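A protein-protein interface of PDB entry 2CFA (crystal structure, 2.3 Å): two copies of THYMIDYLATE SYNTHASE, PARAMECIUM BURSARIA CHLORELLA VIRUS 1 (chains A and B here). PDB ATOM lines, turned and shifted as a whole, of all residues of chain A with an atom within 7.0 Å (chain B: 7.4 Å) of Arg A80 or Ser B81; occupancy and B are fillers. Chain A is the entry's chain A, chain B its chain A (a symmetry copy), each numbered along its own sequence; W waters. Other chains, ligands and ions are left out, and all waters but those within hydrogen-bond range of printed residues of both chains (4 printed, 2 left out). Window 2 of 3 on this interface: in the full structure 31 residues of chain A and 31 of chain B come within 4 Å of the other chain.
N of His B83 lies within hydrogen-bond range of O of Ser B169, at 2.8 Å.
Of the 17 printed residues of chain B, 6 touch a printed residue of chain A. Hydrophobic or aromatic side chains of chain B within 4 Å of the printed part of chain A: His B83 and Phe B84. Along chain B the printed residues that touch a printed residue of chain A span positions 78 to 84. Of the 9 printed residues of chain A, 6 touch a printed residue of chain B. Printed residues of chain A that touch a printed residue of chain B: Arg A78, Arg A80, Ser A81, Phe A82, His A83 and Phe A84. Along chain A the printed residues that touch a printed residue of chain B span positions 78 to 84. Among the printed residues, 9 pairs touch across the chains. Among the printed residues, no Asp or Glu carboxylate lies within 4 Å of a Lys or Arg side-chain nitrogen of the other chain.
Of chain B, only Arg B80, Ser B81, Phe B82 and His B83 come within 4 Å of Arg A80. Printed residues of chain B within 4 Å of Ser A81: Arg B80 (3.6 Å). Of the printed residues of chain B, His A83 touches Arg B80. Of the printed residues of chain B, Phe A84 touches Arg B78 (3.0 Å). Leu B77 touches none of the printed residues of chain A. Printed residues of chain A within 4 Å of Arg B78: Phe A84 (3.0 Å). Of chain A, only Arg A80 (3.6 Å) comes within 4 Å of Ser B81. Of the printed residues of chain A, Phe B84 touches Arg A78. The nearest residue of chain B that does not touch Arg A80 is Phe B84 (5.4 Å). The nearest printed residue of chain A that does not touch Ser B81 is Ser A81 (8.0 Å).
Water W4 lies within hydrogen-bond range of O of Leu A77 (2.7 Å) and O of Leu B77 (2.8 Å). Water W3 lies within hydrogen-bond range of O of Leu B77 (2.7 Å) and O of Leu A77 (2.8 Å). Water W2 lies within hydrogen-bond range of the backbone NH of Phe A84 (2.9 Å) and the guanidinium group of Arg B78 (3.3 Å). Water W1 lies within hydrogen-bond range of N of Phe B84 (2.9 Å) and NH2 of Arg A78 (3.3 Å).
Ser B81 touches Arg A80 (O to NH1, 3.6 Å). O of Ser A81 touches NH1 of Arg B80, 3.6 Å away.
A ring nitrogen (NE2) of His B83 lies close to the guanidinium group of Arg A80 (3.4 Å). NH1 of Arg B80 lies close to NE2 of His A83 (3.4 Å). The backbone carbonyl oxygen (O) of Phe A82 is in hydrogen-bond range of the guanidinium group (NE) of Arg B80. The backbone carbonyl oxygen of Phe B82 is in hydrogen-bond range of the guanidinium group of Arg A80, at 3.0 Å. O of Phe A84 is in hydrogen-bond range of NH2 of Arg B78 (3.0 Å). The guanidinium group (NE) of Arg B80 is in hydrogen-bond range of the backbone carbonyl oxygen (O) of Arg A80. NH2 of Arg A78 sits at hydrogen-bond distance from O of Phe B84, at 3.0 Å.
Arg A78 touches Phe B84, and with the chains exchanged Phe A84 touches Arg B78. Arg A80 touches its own counterpart, Arg B80. Arg A80 touches Ser B81, and with the chains exchanged Ser A81 touches Arg B80. Arg A80 touches His B83, and with the chains exchanged His A83 touches Arg B80. Of the 9 pairs that touch across the chains among the printed residues, 9 have their exchanged pair printed and touching as well.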
ATOM      1  N   VAL A  76     -11.815  20.140 -24.009  1.00  0.00           N
ATOM      2  CA  VAL A  76     -12.438  21.264 -23.328  1.00  0.00           C
ATOM      3  C   VAL A  76     -13.779  21.571 -23.995  1.00  0.00           C
ATOM      4  O   VAL A  76     -14.754  21.865 -23.322  1.00  0.00           O
ATOM      5  CB  VAL A  76     -11.494  22.523 -23.288  1.00  0.00           C
ATOM      6  CG1 VAL A  76     -12.194  23.719 -22.647  1.00  0.00           C
ATOM      7  CG2 VAL A  76     -10.190  22.210 -22.545  1.00  0.00           C
ATOM      8  N   LEU A  77     -13.821  21.492 -25.319  1.00  0.00           N
ATOM      9  CA  LEU A  77     -15.070  21.672 -26.093  1.00  0.00           C
ATOM     10  C   LEU A  77     -16.241  20.805 -25.620  1.00  0.00           C
ATOM     11  O   LEU A  77     -17.404  21.136 -25.888  1.00  0.00           O
ATOM     12  CB  LEU A  77     -14.812  21.402 -27.580  1.00  0.00           C
ATOM     13  CG  LEU A  77     -14.462  22.541 -28.554  1.00  0.00           C
ATOM     14  CD1 LEU A  77     -14.042  23.866 -27.886  1.00  0.00           C
ATOM     15  CD2 LEU A  77     -13.430  22.086 -29.592  1.00  0.00           C
ATOM     16  N   ARG A  78     -15.935  19.699 -24.930  1.00  0.00           N
ATOM     17  CA  ARG A  78     -16.962  18.779 -24.472  1.00  0.00           C
ATOM     18  C   ARG A  78     -17.772  19.315 -23.299  1.00  0.00           C
ATOM     19  O   ARG A  78     -18.863  18.827 -23.032  1.00  0.00           O
ATOM     20  CB  ARG A  78     -16.382  17.386 -24.186  1.00  0.00           C
ATOM     21  CG  ARG A  78     -15.857  16.671 -25.471  1.00  0.00           C
ATOM     22  CD  ARG A  78     -17.014  16.202 -26.362  1.00  0.00           C
ATOM     23  NE  ARG A  78     -17.983  15.443 -25.577  1.00  0.00           N
ATOM     24  CZ  ARG A  78     -17.875  14.152 -25.268  1.00  0.00           C
ATOM     25  NH1 ARG A  78     -16.857  13.423 -25.701  1.00  0.00           N
ATOM     26  NH2 ARG A  78     -18.802  13.586 -24.534  1.00  0.00           N
ATOM     27  N   HIS A  79     -17.248  20.335 -22.621  1.00  0.00           N
ATOM     28  CA  HIS A  79     -18.004  21.001 -21.558  1.00  0.00           C
ATOM     29  C   HIS A  79     -19.016  21.940 -22.169  1.00  0.00           C
ATOM     30  O   HIS A  79     -18.798  23.145 -22.281  1.00  0.00           O
ATOM     31  CB  HIS A  79     -17.065  21.678 -20.545  1.00  0.00           C
ATOM     32  CG  HIS A  79     -16.204  20.700 -19.815  1.00  0.00           C
ATOM     33  ND1 HIS A  79     -16.537  20.202 -18.574  1.00  0.00           N
ATOM     34  CD2 HIS A  79     -15.061  20.072 -20.180  1.00  0.00           C
ATOM     35  CE1 HIS A  79     -15.618  19.333 -18.191  1.00  0.00           C
ATOM     36  NE2 HIS A  79     -14.714  19.232 -19.149  1.00  0.00           N
ATOM     37  N   ARG A  80     -20.153  21.356 -22.537  1.00  0.00           N
ATOM     38  CA  ARG A  80     -21.104  21.991 -23.467  1.00  0.00           C
ATOM     39  C   ARG A  80     -21.987  23.084 -22.850  1.00  0.00           C
ATOM     40  O   ARG A  80     -22.707  23.803 -23.572  1.00  0.00           O
ATOM     41  CB  ARG A  80     -21.921  20.941 -24.246  1.00  0.00           C
ATOM     42  CG  ARG A  80     -22.417  19.766 -23.412  1.00  0.00           C
ATOM     43  CD  ARG A  80     -23.290  18.756 -24.220  1.00  0.00           C
ATOM     44  NE  ARG A  80     -24.602  19.313 -24.563  1.00  0.00           N
ATOM     45  CZ  ARG A  80     -25.623  19.432 -23.713  1.00  0.00           C
ATOM     46  NH1 ARG A  80     -26.768  19.959 -24.113  1.00  0.00           N
ATOM     47  NH2 ARG A  80     -25.510  19.034 -22.455  1.00  0.00           N
ATOM     48  N   SER A  81     -21.906  23.259 -21.534  1.00  0.00           N
ATOM     49  CA  SER A  81     -22.576  24.423 -20.919  1.00  0.00           C
ATOM     50  C   SER A  81     -21.826  25.731 -21.214  1.00  0.00           C
ATOM     51  O   SER A  81     -22.374  26.811 -21.046  1.00  0.00           O
ATOM     52  CB  SER A  81     -22.782  24.232 -19.419  1.00  0.00           C
ATOM     53  OG  SER A  81     -21.536  24.198 -18.749  1.00  0.00           O
ATOM     54  N   PHE A  82     -20.579  25.614 -21.657  1.00  0.00           N
ATOM     55  CA  PHE A  82     -19.736  26.752 -21.990  1.00  0.00           C
ATOM     56  C   PHE A  82     -19.900  27.162 -23.438  1.00  0.00           C
ATOM     57  O   PHE A  82     -20.277  26.364 -24.289  1.00  0.00           O
ATOM     58  CB  PHE A  82     -18.258  26.432 -21.728  1.00  0.00           C
ATOM     59  CG  PHE A  82     -17.891  26.402 -20.272  1.00  0.00           C
ATOM     60  CD1 PHE A  82     -17.965  25.213 -19.547  1.00  0.00           C
ATOM     61  CD2 PHE A  82     -17.473  27.560 -19.620  1.00  0.00           C
ATOM     62  CE1 PHE A  82     -17.617  25.185 -18.183  1.00  0.00           C
ATOM     63  CE2 PHE A  82     -17.134  27.540 -18.262  1.00  0.00           C
ATOM     64  CZ  PHE A  82     -17.206  26.354 -17.548  1.00  0.00           C
ATOM     65  N   HIS A  83     -19.593  28.427 -23.707  1.00  0.00           N
ATOM     66  CA  HIS A  83     -19.604  28.963 -25.058  1.00  0.00           C
ATOM     67  C   HIS A  83     -18.178  29.255 -25.425  1.00  0.00           C
ATOM     68  O   HIS A  83     -17.383  29.718 -24.592  1.00  0.00           O
ATOM     69  CB  HIS A  83     -20.434  30.227 -25.129  1.00  0.00           C
ATOM     70  CG  HIS A  83     -21.800  30.077 -24.547  1.00  0.00           C
ATOM     71  ND1 HIS A  83     -22.055  30.244 -23.207  1.00  0.00           N
ATOM     72  CD2 HIS A  83     -22.983  29.754 -25.116  1.00  0.00           C
ATOM     73  CE1 HIS A  83     -23.343  30.063 -22.979  1.00  0.00           C
ATOM     74  NE2 HIS A  83     -23.927  29.764 -24.122  1.00  0.00           N
ATOM     75  N   PHE A  84     -17.843  28.955 -26.668  1.00  0.00           N
ATOM     76  CA  PHE A  84     -16.472  29.065 -27.120  1.00  0.00           C
ATOM     77  C   PHE A  84     -16.353  29.994 -28.333  1.00  0.00           C
ATOM     78  O   PHE A  84     -17.336  30.333 -28.977  1.00  0.00           O
ATOM     79  CB  PHE A  84     -15.893  27.682 -27.424  1.00  0.00           C
ATOM     80  CG  PHE A  84     -16.012  26.692 -26.281  1.00  0.00           C
ATOM     81  CD1 PHE A  84     -17.113  25.834 -26.191  1.00  0.00           C
ATOM     82  CD2 PHE A  84     -15.024  26.609 -25.306  1.00  0.00           C
ATOM     83  CE1 PHE A  84     -17.228  24.904 -25.138  1.00  0.00           C
ATOM     84  CE2 PHE A  84     -15.117  25.671 -24.261  1.00  0.00           C
ATOM     85  CZ  PHE A  84     -16.219  24.823 -24.173  1.00  0.00           C
ATOM     86  N   PHE B  61     -35.841  12.315 -29.989  1.00  0.00           N
ATOM     87  CA  PHE B  61     -34.409  12.372 -29.768  1.00  0.00           C
ATOM     88  C   PHE B  61     -33.831  11.230 -30.580  1.00  0.00           C
ATOM     89  O   PHE B  61     -34.394  10.133 -30.595  1.00  0.00           O
ATOM     90  CB  PHE B  61     -34.171  12.148 -28.276  1.00  0.00           C
ATOM     91  CG  PHE B  61     -32.763  12.401 -27.791  1.00  0.00           C
ATOM     92  CD1 PHE B  61     -31.855  11.349 -27.658  1.00  0.00           C
ATOM     93  CD2 PHE B  61     -32.377  13.670 -27.347  1.00  0.00           C
ATOM     94  CE1 PHE B  61     -30.574  11.569 -27.123  1.00  0.00           C
ATOM     95  CE2 PHE B  61     -31.082  13.893 -26.823  1.00  0.00           C
ATOM     96  CZ  PHE B  61     -30.197  12.844 -26.712  1.00  0.00           C
ATOM     97  N   LEU B  77     -18.424  19.193 -32.744  1.00  0.00           N
ATOM     98  CA  LEU B  77     -18.483  19.403 -31.280  1.00  0.00           C
ATOM     99  C   LEU B  77     -19.012  20.777 -30.855  1.00  0.00           C
ATOM    100  O   LEU B  77     -19.488  20.934 -29.723  1.00  0.00           O
ATOM    101  CB  LEU B  77     -17.098  19.183 -30.660  1.00  0.00           C
ATOM    102  CG  LEU B  77     -16.681  17.816 -30.091  1.00  0.00           C
ATOM    103  CD1 LEU B  77     -17.580  16.633 -30.506  1.00  0.00           C
ATOM    104  CD2 LEU B  77     -15.203  17.524 -30.377  1.00  0.00           C
ATOM    105  N   ARG B  78     -18.921  21.765 -31.755  1.00  0.00           N
ATOM    106  CA  ARG B  78     -19.350  23.117 -31.445  1.00  0.00           C
ATOM    107  C   ARG B  78     -20.863  23.274 -31.392  1.00  0.00           C
ATOM    108  O   ARG B  78     -21.362  24.235 -30.820  1.00  0.00           O
ATOM    109  CB  ARG B  78     -18.695  24.143 -32.382  1.00  0.00           C
ATOM    110  CG  ARG B  78     -17.149  24.241 -32.191  1.00  0.00           C
ATOM    111  CD  ARG B  78     -16.792  24.949 -30.878  1.00  0.00           C
ATOM    112  NE  ARG B  78     -17.515  26.212 -30.770  1.00  0.00           N
ATOM    113  CZ  ARG B  78     -17.142  27.359 -31.333  1.00  0.00           C
ATOM    114  NH1 ARG B  78     -16.019  27.450 -32.030  1.00  0.00           N
ATOM    115  NH2 ARG B  78     -17.890  28.424 -31.182  1.00  0.00           N
ATOM    116  N   HIS B  79     -21.589  22.314 -31.964  1.00  0.00           N
ATOM    117  CA  HIS B  79     -23.049  22.308 -31.857  1.00  0.00           C
ATOM    118  C   HIS B  79     -23.455  21.792 -30.498  1.00  0.00           C
ATOM    119  O   HIS B  79     -23.793  20.623 -30.322  1.00  0.00           O
ATOM    120  CB  HIS B  79     -23.692  21.543 -33.026  1.00  0.00           C
ATOM    121  CG  HIS B  79     -23.431  22.187 -34.348  1.00  0.00           C
ATOM    122  ND1 HIS B  79     -24.326  23.051 -34.941  1.00  0.00           N
ATOM    123  CD2 HIS B  79     -22.346  22.151 -35.159  1.00  0.00           C
ATOM    124  CE1 HIS B  79     -23.817  23.494 -36.077  1.00  0.00           C
ATOM    125  NE2 HIS B  79     -22.616  22.968 -36.231  1.00  0.00           N
ATOM    126  N   ARG B  80     -23.444  22.710 -29.536  1.00  0.00           N
ATOM    127  CA  ARG B  80     -23.442  22.359 -28.105  1.00  0.00           C
ATOM    128  C   ARG B  80     -24.804  21.934 -27.538  1.00  0.00           C
ATOM    129  O   ARG B  80     -24.892  21.455 -26.388  1.00  0.00           O
ATOM    130  CB  ARG B  80     -22.761  23.449 -27.254  1.00  0.00           C
ATOM    131  CG  ARG B  80     -23.123  24.880 -27.635  1.00  0.00           C
ATOM    132  CD  ARG B  80     -22.463  25.953 -26.715  1.00  0.00           C
ATOM    133  NE  ARG B  80     -23.049  25.961 -25.371  1.00  0.00           N
ATOM    134  CZ  ARG B  80     -24.229  26.497 -25.059  1.00  0.00           C
ATOM    135  NH1 ARG B  80     -24.680  26.446 -23.817  1.00  0.00           N
ATOM    136  NH2 ARG B  80     -24.974  27.085 -25.983  1.00  0.00           N
ATOM    137  N   SER B  81     -25.858  22.049 -28.340  1.00  0.00           N
ATOM    138  CA  SER B  81     -27.150  21.469 -27.919  1.00  0.00           C
ATOM    139  C   SER B  81     -27.145  19.937 -28.023  1.00  0.00           C
ATOM    140  O   SER B  81     -27.998  19.274 -27.451  1.00  0.00           O
ATOM    141  CB  SER B  81     -28.320  22.070 -28.692  1.00  0.00           C
ATOM    142  OG  SER B  81     -28.246  21.711 -30.060  1.00  0.00           O
ATOM    143  N   PHE B  82     -26.175  19.394 -28.749  1.00  0.00           N
ATOM    144  CA  PHE B  82     -26.023  17.959 -28.941  1.00  0.00           C
ATOM    145  C   PHE B  82     -25.160  17.340 -27.862  1.00  0.00           C
ATOM    146  O   PHE B  82     -24.330  18.003 -27.251  1.00  0.00           O
ATOM    147  CB  PHE B  82     -25.403  17.653 -30.312  1.00  0.00           C
ATOM    148  CG  PHE B  82     -26.344  17.854 -31.464  1.00  0.00           C
ATOM    149  CD1 PHE B  82     -26.419  19.088 -32.111  1.00  0.00           C
ATOM    150  CD2 PHE B  82     -27.157  16.815 -31.907  1.00  0.00           C
ATOM    151  CE1 PHE B  82     -27.299  19.275 -33.194  1.00  0.00           C
ATOM    152  CE2 PHE B  82     -28.041  16.997 -32.978  1.00  0.00           C
ATOM    153  CZ  PHE B  82     -28.108  18.224 -33.618  1.00  0.00           C
ATOM    154  N   HIS B  83     -25.362  16.045 -27.649  1.00  0.00           N
ATOM    155  CA  HIS B  83     -24.557  15.271 -26.716  1.00  0.00           C
ATOM    156  C   HIS B  83     -23.741  14.311 -27.533  1.00  0.00           C
ATOM    157  O   HIS B  83     -24.218  13.754 -28.534  1.00  0.00           O
ATOM    158  CB  HIS B  83     -25.438  14.517 -25.743  1.00  0.00           C
ATOM    159  CG  HIS B  83     -26.454  15.377 -25.068  1.00  0.00           C
ATOM    160  ND1 HIS B  83     -27.679  15.651 -25.627  1.00  0.00           N
ATOM    161  CD2 HIS B  83     -26.421  16.042 -23.892  1.00  0.00           C
ATOM    162  CE1 HIS B  83     -28.372  16.422 -24.810  1.00  0.00           C
ATOM    163  NE2 HIS B  83     -27.630  16.673 -23.750  1.00  0.00           N
ATOM    164  N   PHE B  84     -22.496  14.141 -27.124  1.00  0.00           N
ATOM    165  CA  PHE B  84     -21.561  13.344 -27.889  1.00  0.00           C
ATOM    166  C   PHE B  84     -20.974  12.205 -27.049  1.00  0.00           C
ATOM    167  O   PHE B  84     -21.079  12.190 -25.830  1.00  0.00           O
ATOM    168  CB  PHE B  84     -20.455  14.225 -28.474  1.00  0.00           C
ATOM    169  CG  PHE B  84     -20.962  15.402 -29.287  1.00  0.00           C
ATOM    170  CD1 PHE B  84     -21.166  16.649 -28.688  1.00  0.00           C
ATOM    171  CD2 PHE B  84     -21.221  15.268 -30.647  1.00  0.00           C
ATOM    172  CE1 PHE B  84     -21.627  17.751 -29.437  1.00  0.00           C
ATOM    173  CE2 PHE B  84     -21.662  16.365 -31.409  1.00  0.00           C
ATOM    174  CZ  PHE B  84     -21.870  17.603 -30.806  1.00  0.00           C
ATOM    175  N   MET B 168     -23.576  11.282 -31.939  1.00  0.00           N
ATOM    176  CA  MET B 168     -24.148  12.605 -31.870  1.00  0.00           C
ATOM    177  C   MET B 168     -25.623  12.399 -31.593  1.00  0.00           C
ATOM    178  O   MET B 168     -26.315  11.794 -32.394  1.00  0.00           O
ATOM    179  CB  MET B 168     -23.912  13.347 -33.199  1.00  0.00           C
ATOM    180  CG  MET B 168     -24.426  14.772 -33.258  1.00  0.00           C
ATOM    181  SD  MET B 168     -23.942  15.595 -34.806  1.00  0.00           S
ATOM    182  CE  MET B 168     -24.854  17.117 -34.717  1.00  0.00           C
ATOM    183  N   SER B 169     -26.087  12.913 -30.459  1.00  0.00           N
ATOM    184  CA  SER B 169     -27.447  12.714 -29.981  1.00  0.00           C
ATOM    185  C   SER B 169     -28.088  14.066 -29.735  1.00  0.00           C
ATOM    186  O   SER B 169     -27.498  14.930 -29.089  1.00  0.00           O
ATOM    187  CB  SER B 169     -27.454  11.920 -28.658  1.00  0.00           C
ATOM    188  OG  SER B 169     -26.746  10.696 -28.753  1.00  0.00           O
ATOM    189  N   GLY B 170     -29.300  14.243 -30.231  1.00  0.00           N
ATOM    190  CA  GLY B 170     -30.026  15.478 -30.008  1.00  0.00           C
ATOM    191  C   GLY B 170     -31.502  15.372 -30.284  1.00  0.00           C
ATOM    192  O   GLY B 170     -31.955  14.419 -30.923  1.00  0.00           O
ATOM    193  N   THR B 171     -32.263  16.361 -29.827  1.00  0.00           N
ATOM    194  CA  THR B 171     -33.695  16.379 -30.102  1.00  0.00           C
ATOM    195  C   THR B 171     -33.892  16.599 -31.603  1.00  0.00           C
ATOM    196  O   THR B 171     -32.960  17.016 -32.295  1.00  0.00           O
ATOM    197  CB  THR B 171     -34.445  17.480 -29.323  1.00  0.00           C
ATOM    198  OG1 THR B 171     -34.105  18.758 -29.869  1.00  0.00           O
ATOM    199  CG2 THR B 171     -34.111  17.442 -27.833  1.00  0.00           C
ATOM    200  N   ARG B 173     -35.699  18.855 -33.153  1.00  0.00           N
ATOM    201  CA  ARG B 173     -35.428  20.295 -33.269  1.00  0.00           C
ATOM    202  C   ARG B 173     -33.961  20.623 -33.582  1.00  0.00           C
ATOM    203  O   ARG B 173     -33.669  21.412 -34.498  1.00  0.00           O
ATOM    204  CB  ARG B 173     -35.809  21.006 -31.969  1.00  0.00           C
ATOM    205  CG  ARG B 173     -35.770  22.522 -32.082  1.00  0.00           C
ATOM    206  CD  ARG B 173     -34.965  23.129 -30.954  1.00  0.00           C
ATOM    207  NE  ARG B 173     -34.770  24.561 -31.112  1.00  0.00           N
ATOM    208  CZ  ARG B 173     -35.264  25.468 -30.286  1.00  0.00           C
ATOM    209  NH1 ARG B 173     -35.020  26.749 -30.498  1.00  0.00           N
ATOM    210  NH2 ARG B 173     -35.966  25.094 -29.230  1.00  0.00           N
ATOM    211  N   ASP B 174     -33.047  20.017 -32.826  1.00  0.00           N
ATOM    212  CA  ASP B 174     -31.634  20.339 -32.933  1.00  0.00           C
ATOM    213  C   ASP B 174     -31.022  19.829 -34.238  1.00  0.00           C
ATOM    214  O   ASP B 174     -30.171  20.494 -34.836  1.00  0.00           O
ATOM    215  CB  ASP B 174     -30.859  19.840 -31.698  1.00  0.00           C
ATOM    216  CG  ASP B 174     -31.331  20.509 -30.402  1.00  0.00           C
ATOM    217  OD1 ASP B 174     -31.287  19.882 -29.323  1.00  0.00           O
ATOM    218  OD2 ASP B 174     -31.767  21.673 -30.448  1.00  0.00           O
ATOM    219  N   TRP B 175     -31.472  18.648 -34.658  1.00  0.00           N
ATOM    220  CA  TRP B 175     -31.124  18.066 -35.939  1.00  0.00           C
ATOM    221  C   TRP B 175     -31.546  18.919 -37.144  1.00  0.00           C
ATOM    222  O   TRP B 175     -30.776  19.068 -38.100  1.00  0.00           O
ATOM    223  CB  TRP B 175     -31.740  16.663 -36.044  1.00  0.00           C
ATOM    224  CG  TRP B 175     -30.968  15.620 -35.299  1.00  0.00           C
ATOM    225  CD1 TRP B 175     -31.374  14.930 -34.199  1.00  0.00           C
ATOM    226  CD2 TRP B 175     -29.635  15.165 -35.594  1.00  0.00           C
ATOM    227  NE1 TRP B 175     -30.388  14.054 -33.796  1.00  0.00           N
ATOM    228  CE2 TRP B 175     -29.306  14.184 -34.630  1.00  0.00           C
ATOM    229  CE3 TRP B 175     -28.685  15.496 -36.576  1.00  0.00           C
ATOM    230  CZ2 TRP B 175     -28.072  13.523 -34.617  1.00  0.00           C
ATOM    231  CZ3 TRP B 175     -27.452  14.836 -36.559  1.00  0.00           C
ATOM    232  CH2 TRP B 175     -27.165  13.854 -35.580  1.00  0.00           C
ATOM    233  N   TYR B 178     -29.246  21.881 -37.351  1.00  0.00           N
ATOM    234  CA  TYR B 178     -27.883  21.447 -37.639  1.00  0.00           C
ATOM    235  C   TYR B 178     -27.767  21.109 -39.130  1.00  0.00           C
ATOM    236  O   TYR B 178     -26.893  21.633 -39.827  1.00  0.00           O
ATOM    237  CB  TYR B 178     -27.443  20.265 -36.758  1.00  0.00           C
ATOM    238  CG  TYR B 178     -26.191  19.605 -37.298  1.00  0.00           C
ATOM    239  CD1 TYR B 178     -24.920  20.153 -37.060  1.00  0.00           C
ATOM    240  CD2 TYR B 178     -26.276  18.461 -38.087  1.00  0.00           C
ATOM    241  CE1 TYR B 178     -23.769  19.564 -37.592  1.00  0.00           C
ATOM    242  CE2 TYR B 178     -25.131  17.872 -38.620  1.00  0.00           C
ATOM    243  CZ  TYR B 178     -23.891  18.426 -38.370  1.00  0.00           C
ATOM    244  OH  TYR B 178     -22.779  17.815 -38.906  1.00  0.00           O
HETATM  245  O   HOH W   1     -21.625  15.199 -24.518  1.00  0.00           O
HETATM  246  O   HOH W   2     -19.912  28.254 -28.641  1.00  0.00           O
HETATM  247  O   HOH W   3     -19.388  19.723 -27.341  1.00  0.00           O
HETATM  248  O   HOH W   4     -18.669  22.693 -27.655  1.00  0.00           O
